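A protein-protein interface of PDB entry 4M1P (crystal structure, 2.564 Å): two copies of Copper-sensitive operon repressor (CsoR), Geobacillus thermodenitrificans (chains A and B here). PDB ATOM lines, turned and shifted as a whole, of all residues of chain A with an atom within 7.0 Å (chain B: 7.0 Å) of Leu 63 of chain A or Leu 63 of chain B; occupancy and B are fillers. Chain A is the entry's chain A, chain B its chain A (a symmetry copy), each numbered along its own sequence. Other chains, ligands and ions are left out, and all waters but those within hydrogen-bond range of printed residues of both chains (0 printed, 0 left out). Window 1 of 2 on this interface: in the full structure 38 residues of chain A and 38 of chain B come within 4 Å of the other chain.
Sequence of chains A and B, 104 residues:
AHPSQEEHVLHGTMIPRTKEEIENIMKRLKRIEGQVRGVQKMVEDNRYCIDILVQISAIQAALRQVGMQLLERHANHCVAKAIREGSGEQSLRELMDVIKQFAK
N of Arg 64 of chain A lies close to NE2 of Gln 60 of chain B (3.3 Å). The side-chain amide nitrogen (NE2) of Gln 60 of chain A lies close to the backbone NH (N) of Arg 64 of chain B.
Val 36 of chain B touches Leu 29 of chain A. Leu 29 of chain A touches Val 39 of chain B. Val 36 of chain A touches Leu 29 of chain B. Val 39 of chain A touches Leu 29 of chain B. CA of Ser 57 of chain A touches CE1 of Phe 102 of chain B, 3.5 Å away. Gln 60 of chain A touches Leu 63 of chain B. CE1 of Phe 102 of chain B touches OE1 of Gln 60 of chain A, at 3.3 Å. Leu 63 of chain A touches Ile 59 of chain B (CD1 to CG2, 3.5 Å). Leu 63 of chain A touches Leu 63 of chain B. CE1 of Phe 102 of chain A touches OE1 of Gln 60 of chain B, at 3.3 Å.
Leu 29 of chain A touches Val 36 of chain B, and with the chains exchanged Val 36 of chain A touches Leu 29 of chain B. Leu 29 of chain A touches Val 39 of chain B, and with the chains exchanged Val 39 of chain A touches Leu 29 of chain B. Gln 60 of chain A touches Phe 102 of chain B, and with the chains exchanged Phe 102 of chain A touches Gln 60 of chain B. Leu 63 of chain B touches its own counterpart, Leu 63 of chain A. Of the 15 pairs that touch across the chains among the printed residues, 15 have their exchanged pair printed and touching as well.
Leu 63 of chain B touches three residues of chain A. Of the printed residues of chain A, Arg 64 of chain B touches Gln 60 (3.3 Å). Of the printed residues of chain B, Gln 60 of chain A touches Leu 63, Arg 64 and Phe 102. Of the printed residues of chain B, Leu 29 of chain A touches Val 36 and Val 39. Printed residues of chain B within 4 Å of Val 36 of chain A: Leu 29. Ala 62 of chain B touches none of the printed residues of chain A.
Printed residues of chain B that touch a printed residue of chain A: Leu 29, Val 36, Val 39, Ser 57, Ile 59, Gln 60, Leu 63, Arg 64 and Phe 102. Hydrophobic or aromatic side chains of chain B that line the printed part of chain A: Leu 29, Val 36, Val 39, Ile 59, Leu 63 and Phe 102. Along chain B the printed residues that touch a printed residue of chain A span positions 29 to 102. Printed residues of chain A that touch a printed residue of chain B: Leu 29, Val 36, Val 39, Ser 57, Ile 59, Gln 60, Leu 63, Arg 64 and Phe 102. Hydrophobic or aromatic side chains of chain A within 4 Å of the printed part of chain B: Leu 29, Val 36, Val 39, Ile 59, Leu 63 and Phe 102. Among the printed residues, no Asp or Glu carboxylate lies within 4 Å of a Lys or Arg side-chain nitrogen of the other chain.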
ATOM      1  N   LEU A  29      17.540   2.477  11.911  1.00  0.00           N
ATOM      2  CA  LEU A  29      17.450   3.191  13.180  1.00  0.00           C
ATOM      3  C   LEU A  29      18.830   3.632  13.678  1.00  0.00           C
ATOM      4  O   LEU A  29      18.966   4.698  14.289  1.00  0.00           O
ATOM      5  CB  LEU A  29      16.756   2.331  14.234  1.00  0.00           C
ATOM      6  CG  LEU A  29      15.393   1.734  13.879  1.00  0.00           C
ATOM      7  CD1 LEU A  29      14.855   0.920  15.049  1.00  0.00           C
ATOM      8  CD2 LEU A  29      14.402   2.811  13.475  1.00  0.00           C
ATOM      9  N   ILE A  32      19.719   6.598  11.585  1.00  0.00           N
ATOM     10  CA  ILE A  32      18.931   7.672  12.175  1.00  0.00           C
ATOM     11  C   ILE A  32      19.504   8.128  13.525  1.00  0.00           C
ATOM     12  O   ILE A  32      19.590   9.330  13.778  1.00  0.00           O
ATOM     13  CB  ILE A  32      17.447   7.288  12.299  1.00  0.00           C
ATOM     14  CG1 ILE A  32      16.782   7.262  10.922  1.00  0.00           C
ATOM     15  CG2 ILE A  32      16.706   8.274  13.177  1.00  0.00           C
ATOM     16  CD1 ILE A  32      15.300   6.907  10.974  1.00  0.00           C
ATOM     17  N   GLN A  35      22.461  10.283  12.715  1.00  0.00           N
ATOM     18  CA  GLN A  35      21.968  11.580  12.281  1.00  0.00           C
ATOM     19  C   GLN A  35      21.607  12.433  13.489  1.00  0.00           C
ATOM     20  O   GLN A  35      22.012  13.595  13.583  1.00  0.00           O
ATOM     21  CB  GLN A  35      20.755  11.410  11.366  1.00  0.00           C
ATOM     22  CG  GLN A  35      21.050  10.688  10.057  1.00  0.00           C
ATOM     23  CD  GLN A  35      19.811  10.472   9.213  1.00  0.00           C
ATOM     24  OE1 GLN A  35      18.862   9.817   9.639  1.00  0.00           O
ATOM     25  NE2 GLN A  35      19.815  11.024   8.005  1.00  0.00           N
ATOM     26  N   VAL A  36      20.873  11.844  14.429  1.00  0.00           N
ATOM     27  CA  VAL A  36      20.476  12.552  15.644  1.00  0.00           C
ATOM     28  C   VAL A  36      21.678  13.053  16.463  1.00  0.00           C
ATOM     29  O   VAL A  36      21.671  14.182  16.967  1.00  0.00           O
ATOM     30  CB  VAL A  36      19.524  11.705  16.518  1.00  0.00           C
ATOM     31  CG1 VAL A  36      19.202  12.421  17.813  1.00  0.00           C
ATOM     32  CG2 VAL A  36      18.236  11.417  15.760  1.00  0.00           C
ATOM     33  N   VAL A  39      23.427  15.799  14.615  1.00  0.00           N
ATOM     34  CA  VAL A  39      22.726  17.053  14.861  1.00  0.00           C
ATOM     35  C   VAL A  39      23.132  17.608  16.217  1.00  0.00           C
ATOM     36  O   VAL A  39      23.340  18.815  16.369  1.00  0.00           O
ATOM     37  CB  VAL A  39      21.200  16.863  14.765  1.00  0.00           C
ATOM     38  CG1 VAL A  39      20.466  18.069  15.311  1.00  0.00           C
ATOM     39  CG2 VAL A  39      20.807  16.620  13.326  1.00  0.00           C
ATOM     40  N   ILE A  56      17.780  17.944  10.126  1.00  0.00           N
ATOM     41  CA  ILE A  56      16.541  17.557  10.784  1.00  0.00           C
ATOM     42  C   ILE A  56      15.521  17.104   9.747  1.00  0.00           C
ATOM     43  O   ILE A  56      14.808  16.124   9.954  1.00  0.00           O
ATOM     44  CB  ILE A  56      15.972  18.687  11.652  1.00  0.00           C
ATOM     45  CG1 ILE A  56      16.853  18.883  12.891  1.00  0.00           C
ATOM     46  CG2 ILE A  56      14.538  18.378  12.065  1.00  0.00           C
ATOM     47  CD1 ILE A  56      16.290  19.838  13.900  1.00  0.00           C
ATOM     48  N   SER A  57      15.467  17.807   8.623  1.00  0.00           N
ATOM     49  CA  SER A  57      14.570  17.421   7.547  1.00  0.00           C
ATOM     50  C   SER A  57      14.918  16.024   7.049  1.00  0.00           C
ATOM     51  O   SER A  57      14.032  15.207   6.785  1.00  0.00           O
ATOM     52  CB  SER A  57      14.640  18.420   6.400  1.00  0.00           C
ATOM     53  OG  SER A  57      13.795  17.999   5.350  1.00  0.00           O
ATOM     54  N   ALA A  58      16.216  15.754   6.933  1.00  0.00           N
ATOM     55  CA  ALA A  58      16.686  14.426   6.566  1.00  0.00           C
ATOM     56  C   ALA A  58      16.153  13.384   7.548  1.00  0.00           C
ATOM     57  O   ALA A  58      15.554  12.392   7.135  1.00  0.00           O
ATOM     58  CB  ALA A  58      18.202  14.386   6.516  1.00  0.00           C
ATOM     59  N   ILE A  59      16.361  13.622   8.843  1.00  0.00           N
ATOM     60  CA  ILE A  59      15.915  12.690   9.877  1.00  0.00           C
ATOM     61  C   ILE A  59      14.420  12.377   9.799  1.00  0.00           C
ATOM     62  O   ILE A  59      14.043  11.210   9.716  1.00  0.00           O
ATOM     63  CB  ILE A  59      16.273  13.184  11.282  1.00  0.00           C
ATOM     64  CG1 ILE A  59      17.777  13.409  11.379  1.00  0.00           C
ATOM     65  CG2 ILE A  59      15.845  12.164  12.320  1.00  0.00           C
ATOM     66  CD1 ILE A  59      18.230  14.004  12.689  1.00  0.00           C
ATOM     67  N   GLN A  60      13.579  13.409   9.824  1.00  0.00           N
ATOM     68  CA  GLN A  60      12.129  13.235   9.680  1.00  0.00           C
ATOM     69  C   GLN A  60      11.775  12.394   8.451  1.00  0.00           C
ATOM     70  O   GLN A  60      10.897  11.533   8.502  1.00  0.00           O
ATOM     71  CB  GLN A  60      11.431  14.588   9.590  1.00  0.00           C
ATOM     72  CG  GLN A  60      11.400  15.367  10.887  1.00  0.00           C
ATOM     73  CD  GLN A  60      10.711  16.703  10.720  1.00  0.00           C
ATOM     74  OE1 GLN A  60      10.714  17.282   9.632  1.00  0.00           O
ATOM     75  NE2 GLN A  60      10.107  17.197  11.792  1.00  0.00           N
ATOM     76  N   ALA A  61      12.470  12.653   7.353  1.00  0.00           N
ATOM     77  CA  ALA A  61      12.295  11.880   6.132  1.00  0.00           C
ATOM     78  C   ALA A  61      12.617  10.405   6.361  1.00  0.00           C
ATOM     79  O   ALA A  61      11.850   9.530   5.967  1.00  0.00           O
ATOM     80  CB  ALA A  61      13.166  12.444   5.022  1.00  0.00           C
ATOM     81  N   ALA A  62      13.757  10.133   6.987  1.00  0.00           N
ATOM     82  CA  ALA A  62      14.166   8.756   7.245  1.00  0.00           C
ATOM     83  C   ALA A  62      13.196   8.048   8.194  1.00  0.00           C
ATOM     84  O   ALA A  62      13.018   6.835   8.106  1.00  0.00           O
ATOM     85  CB  ALA A  62      15.578   8.711   7.797  1.00  0.00           C
ATOM     86  N   LEU A  63      12.580   8.809   9.098  1.00  0.00           N
ATOM     87  CA  LEU A  63      11.620   8.255  10.045  1.00  0.00           C
ATOM     88  C   LEU A  63      10.293   7.892   9.388  1.00  0.00           C
ATOM     89  O   LEU A  63       9.705   6.856   9.709  1.00  0.00           O
ATOM     90  CB  LEU A  63      11.374   9.225  11.195  1.00  0.00           C
ATOM     91  CG  LEU A  63      12.288   9.046  12.396  1.00  0.00           C
ATOM     92  CD1 LEU A  63      12.022  10.138  13.397  1.00  0.00           C
ATOM     93  CD2 LEU A  63      12.069   7.682  13.022  1.00  0.00           C
ATOM     94  N   ARG A  64       9.817   8.752   8.491  1.00  0.00           N
ATOM     95  CA  ARG A  64       8.622   8.449   7.711  1.00  0.00           C
ATOM     96  C   ARG A  64       8.830   7.158   6.929  1.00  0.00           C
ATOM     97  O   ARG A  64       7.929   6.320   6.832  1.00  0.00           O
ATOM     98  CB  ARG A  64       8.294   9.586   6.747  1.00  0.00           C
ATOM     99  CG  ARG A  64       7.401  10.661   7.328  1.00  0.00           C
ATOM    100  CD  ARG A  64       6.935  11.640   6.250  1.00  0.00           C
ATOM    101  NE  ARG A  64       8.028  12.450   5.711  1.00  0.00           N
ATOM    102  CZ  ARG A  64       8.447  13.594   6.248  1.00  0.00           C
ATOM    103  NH1 ARG A  64       7.874  14.062   7.353  1.00  0.00           N
ATOM    104  NH2 ARG A  64       9.446  14.269   5.689  1.00  0.00           N
ATOM    105  N   GLN A  65      10.033   7.000   6.385  1.00  0.00           N
ATOM    106  CA  GLN A  65      10.370   5.837   5.578  1.00  0.00           C
ATOM    107  C   GLN A  65      10.293   4.561   6.412  1.00  0.00           C
ATOM    108  O   GLN A  65       9.578   3.626   6.060  1.00  0.00           O
ATOM    109  CB  GLN A  65      11.763   6.005   4.965  1.00  0.00           C
ATOM    110  CG  GLN A  65      12.042   5.118   3.759  1.00  0.00           C
ATOM    111  CD  GLN A  65      13.384   5.427   3.112  1.00  0.00           C
ATOM    112  OE1 GLN A  65      13.991   4.572   2.465  1.00  0.00           O
ATOM    113  NE2 GLN A  65      13.851   6.660   3.285  1.00  0.00           N
ATOM    114  N   VAL A  66      11.015   4.521   7.524  1.00  0.00           N
ATOM    115  CA  VAL A  66      10.985   3.327   8.356  1.00  0.00           C
ATOM    116  C   VAL A  66       9.591   3.103   8.960  1.00  0.00           C
ATOM    117  O   VAL A  66       9.143   1.969   9.091  1.00  0.00           O
ATOM    118  CB  VAL A  66      12.105   3.332   9.432  1.00  0.00           C
ATOM    119  CG1 VAL A  66      11.828   4.367  10.504  1.00  0.00           C
ATOM    120  CG2 VAL A  66      12.252   1.962  10.049  1.00  0.00           C
ATOM    121  N   GLY A  67       8.892   4.185   9.287  1.00  0.00           N
ATOM    122  CA  GLY A  67       7.550   4.086   9.834  1.00  0.00           C
ATOM    123  C   GLY A  67       6.550   3.495   8.853  1.00  0.00           C
ATOM    124  O   GLY A  67       5.759   2.609   9.204  1.00  0.00           O
ATOM    125  N   MET A  68       6.578   3.989   7.620  1.00  0.00           N
ATOM    126  CA  MET A  68       5.711   3.465   6.575  1.00  0.00           C
ATOM    127  C   MET A  68       6.018   1.992   6.335  1.00  0.00           C
ATOM    128  O   MET A  68       5.112   1.184   6.132  1.00  0.00           O
ATOM    129  CB  MET A  68       5.898   4.258   5.284  1.00  0.00           C
ATOM    130  CG  MET A  68       4.978   3.845   4.141  1.00  0.00           C
ATOM    131  SD  MET A  68       3.231   4.134   4.508  1.00  0.00           S
ATOM    132  CE  MET A  68       3.308   5.819   5.110  1.00  0.00           C
ATOM    133  N   GLN A  69       7.299   1.643   6.376  1.00  0.00           N
ATOM    134  CA  GLN A  69       7.710   0.274   6.130  1.00  0.00           C
ATOM    135  C   GLN A  69       7.101  -0.643   7.176  1.00  0.00           C
ATOM    136  O   GLN A  69       6.573  -1.706   6.850  1.00  0.00           O
ATOM    137  CB  GLN A  69       9.233   0.154   6.143  1.00  0.00           C
ATOM    138  N   PHE A 102      -0.796   9.220  13.784  1.00  0.00           N
ATOM    139  CA  PHE A 102       0.165   9.831  12.873  1.00  0.00           C
ATOM    140  C   PHE A 102      -0.415  11.087  12.229  1.00  0.00           C
ATOM    141  O   PHE A 102       0.307  11.858  11.597  1.00  0.00           O
ATOM    142  CB  PHE A 102       0.587   8.841  11.786  1.00  0.00           C
ATOM    143  CG  PHE A 102       1.727   7.939  12.184  1.00  0.00           C
ATOM    144  CD1 PHE A 102       2.986   8.463  12.460  1.00  0.00           C
ATOM    145  CD2 PHE A 102       1.550   6.563  12.253  1.00  0.00           C
ATOM    146  CE1 PHE A 102       4.037   7.635  12.814  1.00  0.00           C
ATOM    147  CE2 PHE A 102       2.600   5.729  12.606  1.00  0.00           C
ATOM    148  CZ  PHE A 102       3.843   6.268  12.888  1.00  0.00           C
ATOM    149  N   LEU B  29      17.144  16.742  22.084  1.00  0.00           N
ATOM    150  CA  LEU B  29      17.769  15.783  21.179  1.00  0.00           C
ATOM    151  C   LEU B  29      18.203  14.512  21.916  1.00  0.00           C
ATOM    152  O   LEU B  29      18.143  13.411  21.356  1.00  0.00           O
ATOM    153  CB  LEU B  29      18.962  16.414  20.464  1.00  0.00           C
ATOM    154  CG  LEU B  29      18.734  17.740  19.735  1.00  0.00           C
ATOM    155  CD1 LEU B  29      20.026  18.209  19.080  1.00  0.00           C
ATOM    156  CD2 LEU B  29      17.622  17.626  18.708  1.00  0.00           C
ATOM    157  N   ILE B  32      15.049  12.583  22.467  1.00  0.00           N
ATOM    158  CA  ILE B  32      14.788  11.989  21.163  1.00  0.00           C
ATOM    159  C   ILE B  32      15.749  10.831  20.857  1.00  0.00           C
ATOM    160  O   ILE B  32      15.314   9.788  20.366  1.00  0.00           O
ATOM    161  CB  ILE B  32      14.810  13.043  20.043  1.00  0.00           C
ATOM    162  CG1 ILE B  32      13.573  13.940  20.125  1.00  0.00           C
ATOM    163  CG2 ILE B  32      14.840  12.382  18.680  1.00  0.00           C
ATOM    164  CD1 ILE B  32      13.520  14.997  19.027  1.00  0.00           C
ATOM    165  N   GLN B  35      14.488   7.899  22.822  1.00  0.00           N
ATOM    166  CA  GLN B  35      13.329   7.358  22.130  1.00  0.00           C
ATOM    167  C   GLN B  35      13.775   6.467  20.980  1.00  0.00           C
ATOM    168  O   GLN B  35      13.294   5.340  20.835  1.00  0.00           O
ATOM    169  CB  GLN B  35      12.440   8.491  21.615  1.00  0.00           C
ATOM    170  CG  GLN B  35      11.828   9.358  22.708  1.00  0.00           C
ATOM    171  CD  GLN B  35      11.017  10.513  22.156  1.00  0.00           C
ATOM    172  OE1 GLN B  35      11.536  11.364  21.438  1.00  0.00           O
ATOM    173  NE2 GLN B  35       9.733  10.546  22.492  1.00  0.00           N
ATOM    174  N   VAL B  36      14.719   6.960  20.184  1.00  0.00           N
ATOM    175  CA  VAL B  36      15.243   6.193  19.055  1.00  0.00           C
ATOM    176  C   VAL B  36      15.870   4.855  19.481  1.00  0.00           C
ATOM    177  O   VAL B  36      15.661   3.825  18.830  1.00  0.00           O
ATOM    178  CB  VAL B  36      16.231   7.024  18.205  1.00  0.00           C
ATOM    179  CG1 VAL B  36      16.831   6.181  17.099  1.00  0.00           C
ATOM    180  CG2 VAL B  36      15.521   8.226  17.602  1.00  0.00           C
ATOM    181  N   VAL B  39      13.204   2.529  20.705  1.00  0.00           N
ATOM    182  CA  VAL B  39      12.582   1.881  19.558  1.00  0.00           C
ATOM    183  C   VAL B  39      13.460   0.737  19.077  1.00  0.00           C
ATOM    184  O   VAL B  39      12.965  -0.337  18.728  1.00  0.00           O
ATOM    185  CB  VAL B  39      12.310   2.894  18.429  1.00  0.00           C
ATOM    186  CG1 VAL B  39      11.951   2.188  17.139  1.00  0.00           C
ATOM    187  CG2 VAL B  39      11.195   3.827  18.842  1.00  0.00           C
ATOM    188  N   ILE B  56       7.275   5.684  17.312  1.00  0.00           N
ATOM    189  CA  ILE B  56       7.780   6.407  16.154  1.00  0.00           C
ATOM    190  C   ILE B  56       6.985   7.691  15.954  1.00  0.00           C
ATOM    191  O   ILE B  56       7.551   8.739  15.647  1.00  0.00           O
ATOM    192  CB  ILE B  56       7.757   5.549  14.883  1.00  0.00           C
ATOM    193  CG1 ILE B  56       8.830   4.458  14.975  1.00  0.00           C
ATOM    194  CG2 ILE B  56       7.982   6.411  13.647  1.00  0.00           C
ATOM    195  CD1 ILE B  56       9.018   3.674  13.711  1.00  0.00           C
ATOM    196  N   SER B  57       5.674   7.613  16.150  1.00  0.00           N
ATOM    197  CA  SER B  57       4.835   8.793  16.044  1.00  0.00           C
ATOM    198  C   SER B  57       5.262   9.835  17.070  1.00  0.00           C
ATOM    199  O   SER B  57       5.321  11.032  16.771  1.00  0.00           O
ATOM    200  CB  SER B  57       3.368   8.434  16.239  1.00  0.00           C
ATOM    201  OG  SER B  57       2.579   9.603  16.177  1.00  0.00           O
ATOM    202  N   ALA B  58       5.569   9.371  18.278  1.00  0.00           N
ATOM    203  CA  ALA B  58       6.089  10.246  19.319  1.00  0.00           C
ATOM    204  C   ALA B  58       7.355  10.953  18.836  1.00  0.00           C
ATOM    205  O   ALA B  58       7.444  12.178  18.902  1.00  0.00           O
ATOM    206  CB  ALA B  58       6.366   9.464  20.590  1.00  0.00           C
ATOM    207  N   ILE B  59       8.318  10.178  18.339  1.00  0.00           N
ATOM    208  CA  ILE B  59       9.582  10.735  17.862  1.00  0.00           C
ATOM    209  C   ILE B  59       9.398  11.817  16.797  1.00  0.00           C
ATOM    210  O   ILE B  59       9.897  12.929  16.962  1.00  0.00           O
ATOM    211  CB  ILE B  59      10.526   9.645  17.343  1.00  0.00           C
ATOM    212  CG1 ILE B  59      10.776   8.618  18.440  1.00  0.00           C
ATOM    213  CG2 ILE B  59      11.845  10.257  16.912  1.00  0.00           C
ATOM    214  CD1 ILE B  59      11.604   7.436  18.003  1.00  0.00           C
ATOM    215  N   GLN B  60       8.690  11.495  15.717  1.00  0.00           N
ATOM    216  CA  GLN B  60       8.385  12.472  14.666  1.00  0.00           C
ATOM    217  C   GLN B  60       7.776  13.754  15.239  1.00  0.00           C
ATOM    218  O   GLN B  60       8.117  14.860  14.823  1.00  0.00           O
ATOM    219  CB  GLN B  60       7.435  11.873  13.633  1.00  0.00           C
ATOM    220  CG  GLN B  60       8.058  10.823  12.740  1.00  0.00           C
ATOM    221  CD  GLN B  60       7.057  10.261  11.756  1.00  0.00           C
ATOM    222  OE1 GLN B  60       5.854  10.231  12.027  1.00  0.00           O
ATOM    223  NE2 GLN B  60       7.541   9.822  10.602  1.00  0.00           N
ATOM    224  N   ALA B  61       6.876  13.589  16.198  1.00  0.00           N
ATOM    225  CA  ALA B  61       6.271  14.719  16.888  1.00  0.00           C
ATOM    226  C   ALA B  61       7.328  15.563  17.597  1.00  0.00           C
ATOM    227  O   ALA B  61       7.336  16.785  17.475  1.00  0.00           O
ATOM    228  CB  ALA B  61       5.229  14.233  17.882  1.00  0.00           C
ATOM    229  N   ALA B  62       8.209  14.909  18.347  1.00  0.00           N
ATOM    230  CA  ALA B  62       9.252  15.622  19.078  1.00  0.00           C
ATOM    231  C   ALA B  62      10.223  16.329  18.130  1.00  0.00           C
ATOM    232  O   ALA B  62      10.780  17.369  18.476  1.00  0.00           O
ATOM    233  CB  ALA B  62      10.001  14.677  19.998  1.00  0.00           C
ATOM    234  N   LEU B  63      10.422  15.759  16.942  1.00  0.00           N
ATOM    235  CA  LEU B  63      11.308  16.347  15.944  1.00  0.00           C
ATOM    236  C   LEU B  63      10.713  17.590  15.292  1.00  0.00           C
ATOM    237  O   LEU B  63      11.426  18.568  15.057  1.00  0.00           O
ATOM    238  CB  LEU B  63      11.665  15.326  14.870  1.00  0.00           C
ATOM    239  CG  LEU B  63      12.919  14.512  15.145  1.00  0.00           C
ATOM    240  CD1 LEU B  63      13.084  13.467  14.075  1.00  0.00           C
ATOM    241  CD2 LEU B  63      14.132  15.421  15.196  1.00  0.00           C
ATOM    242  N   ARG B  64       9.418  17.540  14.985  1.00  0.00           N
ATOM    243  CA  ARG B  64       8.717  18.712  14.472  1.00  0.00           C
ATOM    244  C   ARG B  64       8.827  19.857  15.472  1.00  0.00           C
ATOM    245  O   ARG B  64       9.031  21.014  15.094  1.00  0.00           O
ATOM    246  CB  ARG B  64       7.246  18.398  14.212  1.00  0.00           C
ATOM    247  CG  ARG B  64       6.956  17.865  12.826  1.00  0.00           C
ATOM    248  CD  ARG B  64       5.452  17.787  12.562  1.00  0.00           C
ATOM    249  NE  ARG B  64       4.783  16.784  13.390  1.00  0.00           N
ATOM    250  CZ  ARG B  64       4.676  15.496  13.066  1.00  0.00           C
ATOM    251  NH1 ARG B  64       5.207  15.047  11.932  1.00  0.00           N
ATOM    252  NH2 ARG B  64       4.047  14.653  13.876  1.00  0.00           N
ATOM    253  N   GLN B  65       8.706  19.520  16.752  1.00  0.00           N
ATOM    254  CA  GLN B  65       8.751  20.507  17.820  1.00  0.00           C
ATOM    255  C   GLN B  65      10.114  21.195  17.861  1.00  0.00           C
ATOM    256  O   GLN B  65      10.200  22.418  17.785  1.00  0.00           O
ATOM    257  CB  GLN B  65       8.433  19.847  19.164  1.00  0.00           C
ATOM    258  CG  GLN B  65       7.991  20.809  20.260  1.00  0.00           C
ATOM    259  CD  GLN B  65       7.557  20.084  21.525  1.00  0.00           C
ATOM    260  OE1 GLN B  65       7.618  20.633  22.626  1.00  0.00           O
ATOM    261  NE2 GLN B  65       7.114  18.840  21.369  1.00  0.00           N
ATOM    262  N   VAL B  66      11.181  20.416  17.967  1.00  0.00           N
ATOM    263  CA  VAL B  66      12.506  21.017  18.018  1.00  0.00           C
ATOM    264  C   VAL B  66      12.848  21.723  16.697  1.00  0.00           C
ATOM    265  O   VAL B  66      13.488  22.769  16.696  1.00  0.00           O
ATOM    266  CB  VAL B  66      13.598  19.999  18.447  1.00  0.00           C
ATOM    267  CG1 VAL B  66      13.850  18.975  17.358  1.00  0.00           C
ATOM    268  CG2 VAL B  66      14.878  20.716  18.801  1.00  0.00           C
ATOM    269  N   GLY B  67      12.385  21.172  15.579  1.00  0.00           N
ATOM    270  CA  GLY B  67      12.623  21.777  14.279  1.00  0.00           C
ATOM    271  C   GLY B  67      11.953  23.133  14.123  1.00  0.00           C
ATOM    272  O   GLY B  67      12.569  24.099  13.653  1.00  0.00           O
ATOM    273  N   MET B  68      10.684  23.207  14.512  1.00  0.00           N
ATOM    274  CA  MET B  68       9.951  24.464  14.468  1.00  0.00           C
ATOM    275  C   MET B  68      10.621  25.489  15.373  1.00  0.00           C
ATOM    276  O   MET B  68      10.722  26.666  15.027  1.00  0.00           O
ATOM    277  CB  MET B  68       8.503  24.247  14.899  1.00  0.00           C
ATOM    278  CG  MET B  68       7.618  25.487  14.814  1.00  0.00           C
ATOM    279  SD  MET B  68       7.419  26.090  13.121  1.00  0.00           S
ATOM    280  CE  MET B  68       7.002  24.560  12.287  1.00  0.00           C
ATOM    281  N   GLN B  69      11.096  25.033  16.527  1.00  0.00           N
ATOM    282  CA  GLN B  69      11.726  25.927  17.482  1.00  0.00           C
ATOM    283  C   GLN B  69      12.960  26.557  16.861  1.00  0.00           C
ATOM    284  O   GLN B  69      13.173  27.765  16.973  1.00  0.00           O
ATOM    285  CB  GLN B  69      12.099  25.179  18.760  1.00  0.00           C
ATOM    286  N   PHE B 102      11.399  21.025   3.813  1.00  0.00           N
ATOM    287  CA  PHE B 102      10.510  20.381   4.774  1.00  0.00           C
ATOM    288  C   PHE B 102       9.185  19.997   4.121  1.00  0.00           C
ATOM    289  O   PHE B 102       8.390  19.259   4.703  1.00  0.00           O
ATOM    290  CB  PHE B 102      10.249  21.296   5.971  1.00  0.00           C
ATOM    291  CG  PHE B 102      11.290  21.201   7.057  1.00  0.00           C
ATOM    292  CD1 PHE B 102      11.473  20.016   7.763  1.00  0.00           C
ATOM    293  CD2 PHE B 102      12.065  22.303   7.395  1.00  0.00           C
ATOM    294  CE1 PHE B 102      12.419  19.929   8.770  1.00  0.00           C
ATOM    295  CE2 PHE B 102      13.013  22.222   8.403  1.00  0.00           C
ATOM    296  CZ  PHE B 102      13.190  21.033   9.088  1.00  0.00           C
